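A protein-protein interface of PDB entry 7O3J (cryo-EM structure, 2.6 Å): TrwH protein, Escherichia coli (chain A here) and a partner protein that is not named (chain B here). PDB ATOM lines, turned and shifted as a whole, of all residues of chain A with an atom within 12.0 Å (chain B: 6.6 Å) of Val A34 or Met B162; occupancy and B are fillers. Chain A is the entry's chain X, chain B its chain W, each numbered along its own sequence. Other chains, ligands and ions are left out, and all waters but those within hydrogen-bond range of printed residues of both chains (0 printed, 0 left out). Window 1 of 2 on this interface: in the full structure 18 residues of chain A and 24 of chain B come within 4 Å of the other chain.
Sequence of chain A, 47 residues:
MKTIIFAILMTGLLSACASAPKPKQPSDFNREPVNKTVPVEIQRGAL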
ATOM      1  N   GLN A  25      -6.029  21.211 -23.152  1.00  0.00           N
ATOM      2  CA  GLN A  25      -6.635  21.052 -21.838  1.00  0.00           C
ATOM      3  C   GLN A  25      -5.701  20.259 -20.938  1.00  0.00           C
ATOM      4  O   GLN A  25      -5.273  19.164 -21.317  1.00  0.00           O
ATOM      5  CB  GLN A  25      -7.971  20.337 -21.942  1.00  0.00           C
ATOM      6  CG  GLN A  25      -9.133  21.228 -22.322  1.00  0.00           C
ATOM      7  CD  GLN A  25      -9.398  22.308 -21.294  1.00  0.00           C
ATOM      8  OE1 GLN A  25      -9.438  23.493 -21.618  1.00  0.00           O
ATOM      9  NE2 GLN A  25      -9.578  21.902 -20.045  1.00  0.00           N
ATOM     10  N   PRO A  26      -5.347  20.772 -19.766  1.00  0.00           N
ATOM     11  CA  PRO A  26      -4.456  20.025 -18.877  1.00  0.00           C
ATOM     12  C   PRO A  26      -5.106  18.752 -18.362  1.00  0.00           C
ATOM     13  O   PRO A  26      -6.319  18.681 -18.159  1.00  0.00           O
ATOM     14  CB  PRO A  26      -4.188  21.009 -17.738  1.00  0.00           C
ATOM     15  CG  PRO A  26      -5.341  21.921 -17.758  1.00  0.00           C
ATOM     16  CD  PRO A  26      -5.746  22.060 -19.184  1.00  0.00           C
ATOM     17  N   SER A  27      -4.272  17.737 -18.151  1.00  0.00           N
ATOM     18  CA  SER A  27      -4.737  16.467 -17.615  1.00  0.00           C
ATOM     19  C   SER A  27      -5.052  16.617 -16.136  1.00  0.00           C
ATOM     20  O   SER A  27      -4.332  17.305 -15.409  1.00  0.00           O
ATOM     21  CB  SER A  27      -3.681  15.384 -17.823  1.00  0.00           C
ATOM     22  OG  SER A  27      -2.553  15.617 -17.000  1.00  0.00           O
ATOM     23  N   ASP A  28      -6.123  15.965 -15.687  1.00  0.00           N
ATOM     24  CA  ASP A  28      -6.588  16.091 -14.311  1.00  0.00           C
ATOM     25  C   ASP A  28      -6.171  14.916 -13.435  1.00  0.00           C
ATOM     26  O   ASP A  28      -6.931  14.511 -12.548  1.00  0.00           O
ATOM     27  CB  ASP A  28      -8.106  16.264 -14.287  1.00  0.00           C
ATOM     28  CG  ASP A  28      -8.566  17.203 -13.191  1.00  0.00           C
ATOM     29  OD1 ASP A  28      -7.970  17.180 -12.095  1.00  0.00           O
ATOM     30  OD2 ASP A  28      -9.522  17.970 -13.426  1.00  0.00           O
ATOM     31  N   PHE A  29      -4.980  14.364 -13.653  1.00  0.00           N
ATOM     32  CA  PHE A  29      -4.540  13.182 -12.923  1.00  0.00           C
ATOM     33  C   PHE A  29      -3.546  13.520 -11.819  1.00  0.00           C
ATOM     34  O   PHE A  29      -3.719  13.099 -10.671  1.00  0.00           O
ATOM     35  CB  PHE A  29      -3.920  12.179 -13.897  1.00  0.00           C
ATOM     36  CG  PHE A  29      -4.809  11.835 -15.055  1.00  0.00           C
ATOM     37  CD1 PHE A  29      -4.277  11.622 -16.313  1.00  0.00           C
ATOM     38  CD2 PHE A  29      -6.179  11.724 -14.885  1.00  0.00           C
ATOM     39  CE1 PHE A  29      -5.093  11.308 -17.382  1.00  0.00           C
ATOM     40  CE2 PHE A  29      -7.000  11.410 -15.949  1.00  0.00           C
ATOM     41  CZ  PHE A  29      -6.456  11.201 -17.199  1.00  0.00           C
ATOM     42  N   ASN A  30      -2.500  14.275 -12.150  1.00  0.00           N
ATOM     43  CA  ASN A  30      -1.416  14.569 -11.213  1.00  0.00           C
ATOM     44  C   ASN A  30      -1.758  15.829 -10.424  1.00  0.00           C
ATOM     45  O   ASN A  30      -1.125  16.876 -10.557  1.00  0.00           O
ATOM     46  CB  ASN A  30      -0.102  14.724 -11.965  1.00  0.00           C
ATOM     47  CG  ASN A  30      -0.223  15.651 -13.162  1.00  0.00           C
ATOM     48  OD1 ASN A  30      -1.307  15.826 -13.715  1.00  0.00           O
ATOM     49  ND2 ASN A  30       0.889  16.250 -13.564  1.00  0.00           N
ATOM     50  N   ARG A  31      -2.772  15.717  -9.573  1.00  0.00           N
ATOM     51  CA  ARG A  31      -3.237  16.841  -8.770  1.00  0.00           C
ATOM     52  C   ARG A  31      -2.505  16.836  -7.435  1.00  0.00           C
ATOM     53  O   ARG A  31      -2.617  15.880  -6.664  1.00  0.00           O
ATOM     54  CB  ARG A  31      -4.746  16.778  -8.558  1.00  0.00           C
ATOM     55  CG  ARG A  31      -5.282  17.924  -7.732  1.00  0.00           C
ATOM     56  CD  ARG A  31      -6.718  17.687  -7.329  1.00  0.00           C
ATOM     57  NE  ARG A  31      -7.647  17.977  -8.413  1.00  0.00           N
ATOM     58  CZ  ARG A  31      -8.635  18.857  -8.327  1.00  0.00           C
ATOM     59  NH1 ARG A  31      -8.824  19.537  -7.206  1.00  0.00           N
ATOM     60  NH2 ARG A  31      -9.438  19.055  -9.360  1.00  0.00           N
ATOM     61  N   GLU A  32      -1.763  17.901  -7.166  1.00  0.00           N
ATOM     62  CA  GLU A  32      -0.898  17.995  -6.003  1.00  0.00           C
ATOM     63  C   GLU A  32      -0.941  19.411  -5.456  1.00  0.00           C
ATOM     64  O   GLU A  32      -1.290  20.351  -6.176  1.00  0.00           O
ATOM     65  CB  GLU A  32       0.542  17.612  -6.359  1.00  0.00           C
ATOM     66  CG  GLU A  32       1.203  18.563  -7.326  1.00  0.00           C
ATOM     67  CD  GLU A  32       2.595  18.122  -7.702  1.00  0.00           C
ATOM     68  OE1 GLU A  32       3.027  17.057  -7.220  1.00  0.00           O
ATOM     69  OE2 GLU A  32       3.257  18.838  -8.479  1.00  0.00           O
ATOM     70  N   PRO A  33      -0.606  19.594  -4.179  1.00  0.00           N
ATOM     71  CA  PRO A  33      -0.598  20.945  -3.606  1.00  0.00           C
ATOM     72  C   PRO A  33       0.412  21.851  -4.292  1.00  0.00           C
ATOM     73  O   PRO A  33       1.515  21.432  -4.642  1.00  0.00           O
ATOM     74  CB  PRO A  33      -0.224  20.705  -2.142  1.00  0.00           C
ATOM     75  CG  PRO A  33      -0.591  19.302  -1.886  1.00  0.00           C
ATOM     76  CD  PRO A  33      -0.344  18.571  -3.157  1.00  0.00           C
ATOM     77  N   VAL A  34       0.019  23.108  -4.485  1.00  0.00           N
ATOM     78  CA  VAL A  34       0.948  24.097  -5.015  1.00  0.00           C
ATOM     79  C   VAL A  34       1.991  24.465  -3.971  1.00  0.00           C
ATOM     80  O   VAL A  34       3.183  24.576  -4.276  1.00  0.00           O
ATOM     81  CB  VAL A  34       0.190  25.339  -5.510  1.00  0.00           C
ATOM     82  CG1 VAL A  34       1.159  26.366  -6.022  1.00  0.00           C
ATOM     83  CG2 VAL A  34      -0.779  24.965  -6.593  1.00  0.00           C
ATOM     84  N   ASN A  35       1.566  24.659  -2.728  1.00  0.00           N
ATOM     85  CA  ASN A  35       2.434  25.194  -1.683  1.00  0.00           C
ATOM     86  C   ASN A  35       3.092  24.041  -0.941  1.00  0.00           C
ATOM     87  O   ASN A  35       2.475  23.400  -0.090  1.00  0.00           O
ATOM     88  CB  ASN A  35       1.648  26.081  -0.726  1.00  0.00           C
ATOM     89  CG  ASN A  35       1.028  27.265  -1.416  1.00  0.00           C
ATOM     90  OD1 ASN A  35       1.679  28.279  -1.628  1.00  0.00           O
ATOM     91  ND2 ASN A  35      -0.241  27.145  -1.763  1.00  0.00           N
ATOM     92  N   LYS A  36       4.354  23.776  -1.269  1.00  0.00           N
ATOM     93  CA  LYS A  36       5.150  22.862  -0.465  1.00  0.00           C
ATOM     94  C   LYS A  36       5.619  23.519   0.824  1.00  0.00           C
ATOM     95  O   LYS A  36       5.768  22.841   1.844  1.00  0.00           O
ATOM     96  CB  LYS A  36       6.350  22.358  -1.265  1.00  0.00           C
ATOM     97  CG  LYS A  36       6.049  21.173  -2.161  1.00  0.00           C
ATOM     98  CD  LYS A  36       5.316  21.584  -3.421  1.00  0.00           C
ATOM     99  CE  LYS A  36       5.097  20.394  -4.332  1.00  0.00           C
ATOM    100  NZ  LYS A  36       4.273  20.736  -5.517  1.00  0.00           N
ATOM    101  N   THR A  37       5.850  24.828   0.795  1.00  0.00           N
ATOM    102  CA  THR A  37       6.270  25.588   1.960  1.00  0.00           C
ATOM    103  C   THR A  37       5.473  26.879   2.034  1.00  0.00           C
ATOM    104  O   THR A  37       4.979  27.379   1.021  1.00  0.00           O
ATOM    105  CB  THR A  37       7.765  25.913   1.914  1.00  0.00           C
ATOM    106  OG1 THR A  37       8.084  26.510   0.652  1.00  0.00           O
ATOM    107  CG2 THR A  37       8.592  24.654   2.099  1.00  0.00           C
ATOM    108  N   VAL A  38       5.352  27.413   3.239  1.00  0.00           N
ATOM    109  CA  VAL A  38       4.626  28.672   3.434  1.00  0.00           C
ATOM    110  C   VAL A  38       5.414  29.810   2.795  1.00  0.00           C
ATOM    111  O   VAL A  38       6.631  29.921   3.024  1.00  0.00           O
ATOM    112  CB  VAL A  38       4.399  28.932   4.921  1.00  0.00           C
ATOM    113  CG1 VAL A  38       3.483  30.120   5.117  1.00  0.00           C
ATOM    114  CG2 VAL A  38       3.813  27.699   5.577  1.00  0.00           C
ATOM    115  N   PRO A  39       4.787  30.664   1.988  1.00  0.00           N
ATOM    116  CA  PRO A  39       5.514  31.792   1.400  1.00  0.00           C
ATOM    117  C   PRO A  39       6.020  32.744   2.472  1.00  0.00           C
ATOM    118  O   PRO A  39       5.417  32.897   3.533  1.00  0.00           O
ATOM    119  CB  PRO A  39       4.468  32.468   0.507  1.00  0.00           C
ATOM    120  CG  PRO A  39       3.391  31.470   0.328  1.00  0.00           C
ATOM    121  CD  PRO A  39       3.390  30.598   1.532  1.00  0.00           C
ATOM    122  N   VAL A  40       7.150  33.388   2.180  1.00  0.00           N
ATOM    123  CA  VAL A  40       7.698  34.363   3.115  1.00  0.00           C
ATOM    124  C   VAL A  40       6.990  35.707   3.027  1.00  0.00           C
ATOM    125  O   VAL A  40       7.083  36.506   3.965  1.00  0.00           O
ATOM    126  CB  VAL A  40       9.204  34.551   2.888  1.00  0.00           C
ATOM    127  CG1 VAL A  40       9.936  33.255   3.162  1.00  0.00           C
ATOM    128  CG2 VAL A  40       9.463  35.027   1.473  1.00  0.00           C
ATOM    129  N   GLU A  41       6.294  35.986   1.924  1.00  0.00           N
ATOM    130  CA  GLU A  41       5.516  37.216   1.840  1.00  0.00           C
ATOM    131  C   GLU A  41       4.379  37.222   2.849  1.00  0.00           C
ATOM    132  O   GLU A  41       3.950  38.289   3.298  1.00  0.00           O
ATOM    133  CB  GLU A  41       4.970  37.406   0.426  1.00  0.00           C
ATOM    134  CG  GLU A  41       6.029  37.615  -0.642  1.00  0.00           C
ATOM    135  CD  GLU A  41       6.784  36.349  -0.986  1.00  0.00           C
ATOM    136  OE1 GLU A  41       6.245  35.251  -0.745  1.00  0.00           O
ATOM    137  OE2 GLU A  41       7.914  36.451  -1.504  1.00  0.00           O
ATOM    138  N   ILE A  42       3.878  36.040   3.212  1.00  0.00           N
ATOM    139  CA  ILE A  42       2.915  35.906   4.294  1.00  0.00           C
ATOM    140  C   ILE A  42       3.557  36.128   5.655  1.00  0.00           C
ATOM    141  O   ILE A  42       2.858  36.144   6.674  1.00  0.00           O
ATOM    142  CB  ILE A  42       2.253  34.519   4.151  1.00  0.00           C
ATOM    143  CG1 ILE A  42       1.609  34.407   2.773  1.00  0.00           C
ATOM    144  CG2 ILE A  42       1.204  34.262   5.215  1.00  0.00           C
ATOM    145  CD1 ILE A  42       0.760  33.187   2.606  1.00  0.00           C
ATOM    146  N   LEU B 158      -4.419  29.197   1.709  1.00  0.00           N
ATOM    147  CA  LEU B 158      -3.313  28.482   1.088  1.00  0.00           C
ATOM    148  C   LEU B 158      -3.736  27.154   0.477  1.00  0.00           C
ATOM    149  O   LEU B 158      -2.876  26.394   0.028  1.00  0.00           O
ATOM    150  CB  LEU B 158      -2.201  28.247   2.111  1.00  0.00           C
ATOM    151  CG  LEU B 158      -1.440  29.479   2.585  1.00  0.00           C
ATOM    152  CD1 LEU B 158      -0.813  29.217   3.929  1.00  0.00           C
ATOM    153  CD2 LEU B 158      -0.381  29.851   1.582  1.00  0.00           C
ATOM    154  N   TYR B 160      -4.508  25.366  -2.252  1.00  0.00           N
ATOM    155  CA  TYR B 160      -4.439  25.410  -3.705  1.00  0.00           C
ATOM    156  C   TYR B 160      -3.817  24.125  -4.224  1.00  0.00           C
ATOM    157  O   TYR B 160      -2.760  23.708  -3.749  1.00  0.00           O
ATOM    158  CB  TYR B 160      -3.633  26.619  -4.175  1.00  0.00           C
ATOM    159  CG  TYR B 160      -4.443  27.882  -4.226  1.00  0.00           C
ATOM    160  CD1 TYR B 160      -4.684  28.615  -3.083  1.00  0.00           C
ATOM    161  CD2 TYR B 160      -4.981  28.332  -5.414  1.00  0.00           C
ATOM    162  CE1 TYR B 160      -5.431  29.759  -3.122  1.00  0.00           C
ATOM    163  CE2 TYR B 160      -5.729  29.476  -5.460  1.00  0.00           C
ATOM    164  CZ  TYR B 160      -5.949  30.184  -4.312  1.00  0.00           C
ATOM    165  OH  TYR B 160      -6.696  31.331  -4.359  1.00  0.00           O
ATOM    166  N   MET B 161      -4.479  23.503  -5.191  1.00  0.00           N
ATOM    167  CA  MET B 161      -3.983  22.326  -5.884  1.00  0.00           C
ATOM    168  C   MET B 161      -3.688  22.673  -7.335  1.00  0.00           C
ATOM    169  O   MET B 161      -4.140  23.689  -7.861  1.00  0.00           O
ATOM    170  CB  MET B 161      -4.992  21.177  -5.818  1.00  0.00           C
ATOM    171  CG  MET B 161      -5.481  20.836  -4.432  1.00  0.00           C
ATOM    172  SD  MET B 161      -4.156  20.593  -3.245  1.00  0.00           S
ATOM    173  CE  MET B 161      -4.764  21.526  -1.844  1.00  0.00           C
ATOM    174  N   MET B 162      -2.916  21.809  -7.985  1.00  0.00           N
ATOM    175  CA  MET B 162      -2.586  22.024  -9.383  1.00  0.00           C
ATOM    176  C   MET B 162      -2.469  20.688 -10.096  1.00  0.00           C
ATOM    177  O   MET B 162      -2.026  19.701  -9.510  1.00  0.00           O
ATOM    178  CB  MET B 162      -1.290  22.818  -9.544  1.00  0.00           C
ATOM    179  CG  MET B 162      -0.066  22.140  -8.985  1.00  0.00           C
ATOM    180  SD  MET B 162       1.419  23.101  -9.281  1.00  0.00           S
ATOM    181  CE  MET B 162       2.611  22.148  -8.357  1.00  0.00           C
ATOM    182  N   SER B 163      -2.877  20.673 -11.360  1.00  0.00           N
ATOM    183  CA  SER B 163      -2.736  19.511 -12.218  1.00  0.00           C
ATOM    184  C   SER B 163      -2.436  19.986 -13.629  1.00  0.00           C
ATOM    185  O   SER B 163      -2.968  21.003 -14.073  1.00  0.00           O
ATOM    186  CB  SER B 163      -3.999  18.651 -12.208  1.00  0.00           C
ATOM    187  OG  SER B 163      -5.042  19.273 -12.927  1.00  0.00           O
ATOM    188  N   GLY B 164      -1.577  19.253 -14.328  1.00  0.00           N
ATOM    189  CA  GLY B 164      -1.214  19.626 -15.677  1.00  0.00           C
ATOM    190  C   GLY B 164       0.279  19.660 -15.910  1.00  0.00           C
ATOM    191  O   GLY B 164       1.001  18.759 -15.479  1.00  0.00           O
ATOM    192  N   LYS B 166       3.567  20.733 -14.979  1.00  0.00           N
ATOM    193  CA  LYS B 166       4.177  21.272 -13.769  1.00  0.00           C
ATOM    194  C   LYS B 166       5.430  22.089 -14.037  1.00  0.00           C
ATOM    195  O   LYS B 166       5.955  22.702 -13.104  1.00  0.00           O
ATOM    196  CB  LYS B 166       4.516  20.142 -12.807  1.00  0.00           C
ATOM    197  CG  LYS B 166       3.355  19.232 -12.507  1.00  0.00           C
ATOM    198  CD  LYS B 166       2.290  19.950 -11.727  1.00  0.00           C
ATOM    199  CE  LYS B 166       1.108  19.043 -11.490  1.00  0.00           C
ATOM    200  NZ  LYS B 166       1.475  17.898 -10.620  1.00  0.00           N
ATOM    201  N   ALA B 169       4.651  25.715 -13.426  1.00  0.00           N
ATOM    202  CA  ALA B 169       3.909  25.873 -12.190  1.00  0.00           C
ATOM    203  C   ALA B 169       4.533  26.944 -11.301  1.00  0.00           C
ATOM    204  O   ALA B 169       5.748  27.147 -11.323  1.00  0.00           O
ATOM    205  CB  ALA B 169       3.859  24.555 -11.434  1.00  0.00           C
ATOM    206  N   PRO B 170       3.721  27.642 -10.515  1.00  0.00           N
ATOM    207  CA  PRO B 170       4.271  28.545  -9.505  1.00  0.00           C
ATOM    208  C   PRO B 170       4.816  27.764  -8.323  1.00  0.00           C
ATOM    209  O   PRO B 170       4.454  26.611  -8.084  1.00  0.00           O
ATOM    210  CB  PRO B 170       3.070  29.401  -9.091  1.00  0.00           C
ATOM    211  CG  PRO B 170       1.953  29.012  -9.982  1.00  0.00           C
ATOM    212  CD  PRO B 170       2.254  27.667 -10.521  1.00  0.00           C
ATOM    213  N   VAL B 171       5.706  28.411  -7.575  1.00  0.00           N
ATOM    214  CA  VAL B 171       6.212  27.786  -6.362  1.00  0.00           C
ATOM    215  C   VAL B 171       5.292  28.022  -5.177  1.00  0.00           C
ATOM    216  O   VAL B 171       5.370  27.286  -4.189  1.00  0.00           O
ATOM    217  CB  VAL B 171       7.630  28.276  -6.033  1.00  0.00           C
ATOM    218  CG1 VAL B 171       8.577  27.903  -7.144  1.00  0.00           C
ATOM    219  CG2 VAL B 171       7.643  29.767  -5.820  1.00  0.00           C
ATOM    220  N   ASN B 172       4.418  29.021  -5.252  1.00  0.00           N
ATOM    221  CA  ASN B 172       3.491  29.331  -4.179  1.00  0.00           C
ATOM    222  C   ASN B 172       2.266  30.007  -4.771  1.00  0.00           C
ATOM    223  O   ASN B 172       2.383  30.800  -5.705  1.00  0.00           O
ATOM    224  CB  ASN B 172       4.128  30.245  -3.132  1.00  0.00           C
ATOM    225  CG  ASN B 172       4.963  29.490  -2.134  1.00  0.00           C
ATOM    226  OD1 ASN B 172       6.134  29.794  -1.933  1.00  0.00           O
ATOM    227  ND2 ASN B 172       4.368  28.495  -1.498  1.00  0.00           N
ATOM    228  N   ALA B 173       1.099  29.688  -4.227  1.00  0.00           N
ATOM    229  CA  ALA B 173      -0.133  30.372  -4.580  1.00  0.00           C
ATOM    230  C   ALA B 173      -0.969  30.547  -3.326  1.00  0.00           C
ATOM    231  O   ALA B 173      -1.048  29.643  -2.495  1.00  0.00           O
ATOM    232  CB  ALA B 173      -0.926  29.613  -5.643  1.00  0.00           C
ATOM    233  N   PHE B 182       0.200  34.370  -7.268  1.00  0.00           N
ATOM    234  CA  PHE B 182       1.018  33.253  -7.718  1.00  0.00           C
ATOM    235  C   PHE B 182       2.468  33.711  -7.734  1.00  0.00           C
ATOM    236  O   PHE B 182       2.795  34.696  -8.396  1.00  0.00           O
ATOM    237  CB  PHE B 182       0.603  32.785  -9.111  1.00  0.00           C
ATOM    238  CG  PHE B 182      -0.863  32.537  -9.262  1.00  0.00           C
ATOM    239  CD1 PHE B 182      -1.407  31.314  -8.939  1.00  0.00           C
ATOM    240  CD2 PHE B 182      -1.696  33.521  -9.750  1.00  0.00           C
ATOM    241  CE1 PHE B 182      -2.745  31.086  -9.086  1.00  0.00           C
ATOM    242  CE2 PHE B 182      -3.037  33.290  -9.898  1.00  0.00           C
ATOM    243  CZ  PHE B 182      -3.559  32.074  -9.566  1.00  0.00           C
ATOM    244  N   LYS B 183       3.332  32.997  -7.020  1.00  0.00           N
ATOM    245  CA  LYS B 183       4.751  33.319  -6.966  1.00  0.00           C
ATOM    246  C   LYS B 183       5.530  32.343  -7.833  1.00  0.00           C
ATOM    247  O   LYS B 183       5.332  31.131  -7.739  1.00  0.00           O
ATOM    248  CB  LYS B 183       5.285  33.278  -5.537  1.00  0.00           C
ATOM    249  CG  LYS B 183       6.512  34.135  -5.360  1.00  0.00           C
ATOM    250  CD  LYS B 183       7.579  33.477  -4.531  1.00  0.00           C
ATOM    251  CE  LYS B 183       7.104  33.199  -3.137  1.00  0.00           C
ATOM    252  NZ  LYS B 183       8.201  32.615  -2.324  1.00  0.00           N
ATOM    253  N   LEU B 235      -1.665  24.429 -17.259  1.00  0.00           N
ATOM    254  CA  LEU B 235      -1.709  23.971 -15.882  1.00  0.00           C
ATOM    255  C   LEU B 235      -2.949  24.548 -15.227  1.00  0.00           C
ATOM    256  O   LEU B 235      -3.218  25.744 -15.357  1.00  0.00           O
ATOM    257  CB  LEU B 235      -0.453  24.401 -15.125  1.00  0.00           C
ATOM    258  CG  LEU B 235      -0.370  24.075 -13.642  1.00  0.00           C
ATOM    259  CD1 LEU B 235       0.200  22.706 -13.432  1.00  0.00           C
ATOM    260  CD2 LEU B 235       0.477  25.100 -12.963  1.00  0.00           C
ATOM    261  N   ALA B 236      -3.702  23.708 -14.530  1.00  0.00           N
ATOM    262  CA  ALA B 236      -4.915  24.130 -13.852  1.00  0.00           C
ATOM    263  C   ALA B 236      -4.652  24.293 -12.364  1.00  0.00           C
ATOM    264  O   ALA B 236      -4.003  23.453 -11.744  1.00  0.00           O
ATOM    265  CB  ALA B 236      -6.040  23.123 -14.074  1.00  0.00           C
ATOM    266  N   ILE B 237      -5.148  25.389 -11.798  1.00  0.00           N
ATOM    267  CA  ILE B 237      -5.016  25.682 -10.378  1.00  0.00           C
ATOM    268  C   ILE B 237      -6.408  25.656  -9.776  1.00  0.00           C
ATOM    269  O   ILE B 237      -7.333  26.265 -10.320  1.00  0.00           O
ATOM    270  CB  ILE B 237      -4.349  27.047 -10.130  1.00  0.00           C
ATOM    271  CG1 ILE B 237      -3.058  27.184 -10.933  1.00  0.00           C
ATOM    272  CG2 ILE B 237      -4.049  27.215  -8.661  1.00  0.00           C
ATOM    273  CD1 ILE B 237      -1.929  26.357 -10.414  1.00  0.00           C
ATOM    274  N   PHE B 238      -6.561  24.948  -8.664  1.00  0.00           N
ATOM    275  CA  PHE B 238      -7.855  24.771  -8.025  1.00  0.00           C
ATOM    276  C   PHE B 238      -7.821  25.365  -6.629  1.00  0.00           C
ATOM    277  O   PHE B 238      -6.977  24.991  -5.813  1.00  0.00           O
ATOM    278  CB  PHE B 238      -8.231  23.294  -7.961  1.00  0.00           C
ATOM    279  CG  PHE B 238      -8.236  22.623  -9.295  1.00  0.00           C
ATOM    280  CD1 PHE B 238      -9.329  22.720 -10.125  1.00  0.00           C
ATOM    281  CD2 PHE B 238      -7.139  21.910  -9.726  1.00  0.00           C
ATOM    282  CE1 PHE B 238      -9.332  22.111 -11.352  1.00  0.00           C
ATOM    283  CE2 PHE B 238      -7.138  21.302 -10.954  1.00  0.00           C
ATOM    284  CZ  PHE B 238      -8.235  21.404 -11.766  1.00  0.00           C
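Along chain A the printed residues that touch a printed residue of chain B span positions 26 to 42.
Among the printed residues, 35 pairs touch across the chains.
Among the printed residues, Asp or Glu carboxylates within 4 Å of a Lys or Arg side-chain nitrogen of the other chain: Glu A32 with Lys B166 and Glu A41 with Lys B183.
Among the printed residues, pairs that only touch across the chains: Pro A26 with Ser B163 (3.9 Å), Pro A26 with Gly B164 (3.9 Å), Pro A26 with Ala B236 (3.9 Å), Ser A27 with Gly B164 (3.5 Å), Asp A28 with Ser B163 (3.7 Å), Asn A30 with Ser B163 (3.5 Å), Arg A31 with Met B161 (3.8 Å), Arg A31 with Met B162 (3.2 Å), Arg A31 with Ser B163 (3.96 Å), Arg A31 with Phe B238 (3.6 Å), Glu A32 with Met B161 (3.4 Å), Pro A33 with Tyr B160 (3.5 Å), Pro A33 with Met B161 (3.6 Å), Pro A33 with Met B162 (3.9 Å), Val A34 with Met B161 (3.8 Å), Val A34 with Met B162 (3.7 Å), Val A34 with Pro B170 (3.9 Å), Val A34 with Ala B173 (3.8 Å), Lys A36 with Met B162 (3.6 Å), Pro A39 with Leu B158 (3.8 Å), Pro A39 with Asn B172 (3.5 Å) and Ile A42 with Leu B158 (3.7 Å).
O of Pro A33 is in hydrogen-bond range of NZ of Lys A36.
O of Met B161 is in hydrogen-bond range of N of Phe B238 (2.8 Å).
The backbone carbonyl oxygen (O) of Asn B172 sits at hydrogen-bond distance from the backbone NH (N) of Lys B183, 2.7 Å away.
OE2 of Glu A32 lies within salt-bridge range of NZ of Lys A36 (3.7 Å).
The guanidinium group (NH2) of Arg A31 lies within salt-bridge range of the side-chain carboxylate (OD1) of Asp A28 (3.6 Å).
The backbone NH (N) of Ala B236 is in hydrogen-bond range of the backbone carbonyl oxygen (O) of Ser B163 (2.8 Å).
Printed residues of chain B within 4 Å of Asn A30: Met B162 (3.1 Å), Ser B163 (3.5 Å), Gly B164 (3.2 Å) and Lys B166 (2.8 Å).
Of the printed residues of chain B, Pro A33 touches Tyr B160, Met B161 and Met B162.
Of the printed residues of chain B, Glu A41 touches Lys B183.
Met B161 touches just these residues of chain A: Arg A31 (3.8 Å), Glu A32 (3.4 Å), Pro A33 (3.6 Å) and Val A34 (3.8 Å).
Of chain A, only Pro A26, Ser A27, Asp A28, Asn A30 and Arg A31 come within 4 Å of Ser B163.
Of chain A, only Pro A26 (3.9 Å), Ser A27 (3.5 Å) and Asn A30 (3.2 Å) come within 4 Å of Gly B164.
Of chain A, only Val A34 comes within 4 Å of Pro B170.
Of the printed residues of chain A, Val B171 touches Val A34 (3.5 Å).
Phe B182 touches none of the printed residues of chain A.
No residue of chain A comes within 4 Å of Leu B235.
Of chain A, only Pro A26 (3.9 Å) comes within 4 Å of Ala B236.
No residue of chain A comes within 4 Å of Ile B237.
The nearest residue of chain A that does not touch Met B162 is Asn A35 (6.3 Å).
The backbone carbonyl oxygen (O) of Gly B164 sits at hydrogen-bond distance from the side-chain amide nitrogen (ND2) of Asn A30 (3.2 Å).
The backbone carbonyl oxygen (O) of Val A34 sits close to the backbone carbonyl oxygen (O) of Val B171 (3.5 Å).
The side-chain carboxylate (OE2) of Glu A32 is in salt-bridge range of the side-chain amino group (NZ) of Lys B166, 2.9 Å away.
O of Thr A37 lies within hydrogen-bond range of ND2 of Asn B172, at 2.8 Å.
OG of Ser B163 lies within hydrogen-bond range of O of Ser A27, at 3.2 Å.
The backbone NH of Met B162 lies within hydrogen-bond range of the backbone carbonyl oxygen of Glu A32, 2.8 Å away.
The side-chain amino group (NZ) of Lys B183 lies within salt-bridge range of the side-chain carboxylate (OE1) of Glu A41, 3.6 Å away.
The backbone carbonyl oxygen (O) of Asn A30 lies close to the backbone carbonyl oxygen (O) of Met B162 (3.1 Å).
N of Val A34 lies within hydrogen-bond range of O of Tyr B160 (2.9 Å).
O of Ala B173 lies within hydrogen-bond range of ND2 of Asn A35, 2.7 Å away.
NZ of Lys B166 sits at hydrogen-bond distance from O of Asn A30 (2.8 Å).
The side-chain amide nitrogen (ND2) of Asn B172 lies within hydrogen-bond range of the side-chain amide oxygen (OD1) of Asn A35 (2.7 Å).
O of Leu B158 is in hydrogen-bond range of ND2 of Asn A35 (3.3 Å).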
